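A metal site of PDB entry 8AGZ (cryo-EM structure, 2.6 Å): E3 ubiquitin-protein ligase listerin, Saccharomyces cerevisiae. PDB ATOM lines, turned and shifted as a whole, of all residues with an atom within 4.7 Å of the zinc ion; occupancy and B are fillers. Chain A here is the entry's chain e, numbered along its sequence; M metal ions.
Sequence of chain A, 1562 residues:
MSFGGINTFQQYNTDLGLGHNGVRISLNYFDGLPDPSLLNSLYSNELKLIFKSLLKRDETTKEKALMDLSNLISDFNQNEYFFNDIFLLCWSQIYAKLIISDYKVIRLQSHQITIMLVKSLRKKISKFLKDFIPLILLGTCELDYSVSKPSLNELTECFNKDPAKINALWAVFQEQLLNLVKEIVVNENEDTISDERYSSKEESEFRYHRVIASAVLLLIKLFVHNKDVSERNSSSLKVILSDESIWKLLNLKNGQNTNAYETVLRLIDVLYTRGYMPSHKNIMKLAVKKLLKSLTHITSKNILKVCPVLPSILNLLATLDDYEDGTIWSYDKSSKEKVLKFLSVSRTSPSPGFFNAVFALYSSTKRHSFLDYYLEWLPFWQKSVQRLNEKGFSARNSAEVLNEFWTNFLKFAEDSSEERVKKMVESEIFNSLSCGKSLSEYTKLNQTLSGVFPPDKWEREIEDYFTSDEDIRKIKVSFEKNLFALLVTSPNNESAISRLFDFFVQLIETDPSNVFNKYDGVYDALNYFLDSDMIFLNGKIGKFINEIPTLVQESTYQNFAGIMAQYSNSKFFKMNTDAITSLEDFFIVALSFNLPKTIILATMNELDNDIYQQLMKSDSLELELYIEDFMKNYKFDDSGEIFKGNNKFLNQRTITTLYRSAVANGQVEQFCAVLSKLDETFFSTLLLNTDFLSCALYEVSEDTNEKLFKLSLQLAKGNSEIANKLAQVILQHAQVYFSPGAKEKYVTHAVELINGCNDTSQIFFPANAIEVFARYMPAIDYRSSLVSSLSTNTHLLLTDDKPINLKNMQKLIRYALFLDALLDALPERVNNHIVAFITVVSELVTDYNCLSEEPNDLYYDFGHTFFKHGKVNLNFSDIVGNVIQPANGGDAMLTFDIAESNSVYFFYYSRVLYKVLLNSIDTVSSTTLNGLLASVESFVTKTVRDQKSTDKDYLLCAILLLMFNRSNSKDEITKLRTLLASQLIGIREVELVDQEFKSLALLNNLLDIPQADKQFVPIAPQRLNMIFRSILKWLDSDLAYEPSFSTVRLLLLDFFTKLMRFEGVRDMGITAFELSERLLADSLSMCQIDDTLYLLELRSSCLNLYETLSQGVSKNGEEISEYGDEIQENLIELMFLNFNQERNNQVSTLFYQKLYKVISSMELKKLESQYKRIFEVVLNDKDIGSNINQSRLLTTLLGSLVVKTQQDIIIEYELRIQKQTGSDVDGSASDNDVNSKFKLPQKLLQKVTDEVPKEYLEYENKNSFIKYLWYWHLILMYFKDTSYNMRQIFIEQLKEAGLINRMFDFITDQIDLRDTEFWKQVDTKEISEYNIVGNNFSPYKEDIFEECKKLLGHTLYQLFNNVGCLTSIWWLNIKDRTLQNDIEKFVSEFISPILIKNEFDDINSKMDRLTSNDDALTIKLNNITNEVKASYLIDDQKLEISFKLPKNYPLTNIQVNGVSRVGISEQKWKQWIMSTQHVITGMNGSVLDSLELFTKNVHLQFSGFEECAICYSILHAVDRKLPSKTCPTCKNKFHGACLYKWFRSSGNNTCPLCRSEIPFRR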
ATOM      1  N   CYS A1527       6.762  20.043 -11.013  1.00  0.00           N
ATOM      2  CA  CYS A1527       8.197  20.261 -10.858  1.00  0.00           C
ATOM      3  C   CYS A1527       8.469  21.607 -11.523  1.00  0.00           C
ATOM      4  O   CYS A1527       7.956  21.872 -12.588  1.00  0.00           O
ATOM      5  CB  CYS A1527       8.987  19.117 -11.497  1.00  0.00           C
ATOM      6  SG  CYS A1527      10.617  19.490 -12.181  1.00  0.00           S
ATOM      7  N   THR A1529      11.126  23.030 -13.010  1.00  0.00           N
ATOM      8  CA  THR A1529      11.865  23.056 -14.275  1.00  0.00           C
ATOM      9  C   THR A1529      10.976  22.733 -15.458  1.00  0.00           C
ATOM     10  O   THR A1529      11.060  23.371 -16.511  1.00  0.00           O
ATOM     11  CB  THR A1529      13.049  22.072 -14.250  1.00  0.00           C
ATOM     12  OG1 THR A1529      13.822  22.280 -13.067  1.00  0.00           O
ATOM     13  CG2 THR A1529      13.937  22.239 -15.475  1.00  0.00           C
ATOM     14  N   CYS A1530      10.092  21.762 -15.301  1.00  0.00           N
ATOM     15  CA  CYS A1530       9.213  21.365 -16.398  1.00  0.00           C
ATOM     16  C   CYS A1530       7.812  21.881 -16.154  1.00  0.00           C
ATOM     17  O   CYS A1530       7.216  21.625 -15.122  1.00  0.00           O
ATOM     18  CB  CYS A1530       9.244  19.842 -16.608  1.00  0.00           C
ATOM     19  SG  CYS A1530       8.916  18.811 -15.151  1.00  0.00           S
ATOM     20  N   CYS A1551      12.147  14.228 -10.452  1.00  0.00           N
ATOM     21  CA  CYS A1551      11.126  14.255 -11.484  1.00  0.00           C
ATOM     22  C   CYS A1551      11.405  13.241 -12.590  1.00  0.00           C
ATOM     23  O   CYS A1551      12.559  13.039 -12.962  1.00  0.00           O
ATOM     24  CB  CYS A1551      11.010  15.689 -11.995  1.00  0.00           C
ATOM     25  SG  CYS A1551      10.320  15.914 -13.635  1.00  0.00           S
ATOM     26  N   LEU A1553      10.407  13.457 -15.877  1.00  0.00           N
ATOM     27  CA  LEU A1553      10.783  14.148 -17.112  1.00  0.00           C
ATOM     28  C   LEU A1553      12.170  14.747 -17.059  1.00  0.00           C
ATOM     29  O   LEU A1553      12.917  14.675 -18.033  1.00  0.00           O
ATOM     30  CB  LEU A1553       9.762  15.236 -17.449  1.00  0.00           C
ATOM     31  CG  LEU A1553       8.307  14.826 -17.682  1.00  0.00           C
ATOM     32  CD1 LEU A1553       7.525  16.022 -18.200  1.00  0.00           C
ATOM     33  CD2 LEU A1553       8.230  13.670 -18.658  1.00  0.00           C
ATOM     34  N   CYS A1554      12.502  15.358 -15.933  1.00  0.00           N
ATOM     35  CA  CYS A1554      13.807  15.984 -15.787  1.00  0.00           C
ATOM     36  C   CYS A1554      14.416  15.655 -14.431  1.00  0.00           C
ATOM     37  O   CYS A1554      13.714  15.598 -13.440  1.00  0.00           O
ATOM     38  CB  CYS A1554      13.683  17.501 -15.946  1.00  0.00           C
ATOM     39  SG  CYS A1554      13.194  18.353 -14.423  1.00  0.00           S
ATOM     40  N   SER A1556      15.992  17.428 -12.563  1.00  0.00           N
ATOM     41  CA  SER A1556      15.899  18.565 -11.659  1.00  0.00           C
ATOM     42  C   SER A1556      14.836  18.317 -10.599  1.00  0.00           C
ATOM     43  O   SER A1556      13.748  17.827 -10.902  1.00  0.00           O
ATOM     44  CB  SER A1556      15.575  19.845 -12.450  1.00  0.00           C
ATOM     45  OG  SER A1556      15.377  20.945 -11.577  1.00  0.00           O
HETATM   46 ZN    ZN M   1      10.894  18.132 -14.076  1.00  0.00          ZN
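The side-chain sulfur of Cys 1554 lies close to the backbone NH of Ser 1556, 3.5 Å away. N of Thr 1529 sits close to SG of Cys 1527 (3.7 Å). The side-chain sulfur of Cys 1527 lies close to the backbone carbonyl oxygen of Ser 1556 (3.8 Å). The side-chain sulfur (SG) of Cys 1551 lies close to the backbone NH (N) of Leu 1553.
Within 4 Å of the zinc ion: Cys 1527, Cys 1530, Cys 1551 and Cys 1554. Along chain A the residues within 4 Å of the zinc ion span positions 1527 to 1554.
The zinc ion is bound by SG of Cys 1551, 2.3 Å away. The zinc ion is bound by the side-chain sulfur (SG) of Cys 1554 (2.3 Å). The side-chain sulfur (SG) of Cys 1527 is bound to the zinc ion (2.3 Å). The zinc ion is bound by SG of Cys 1530. The zinc ion has four donor atoms within binding distance.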
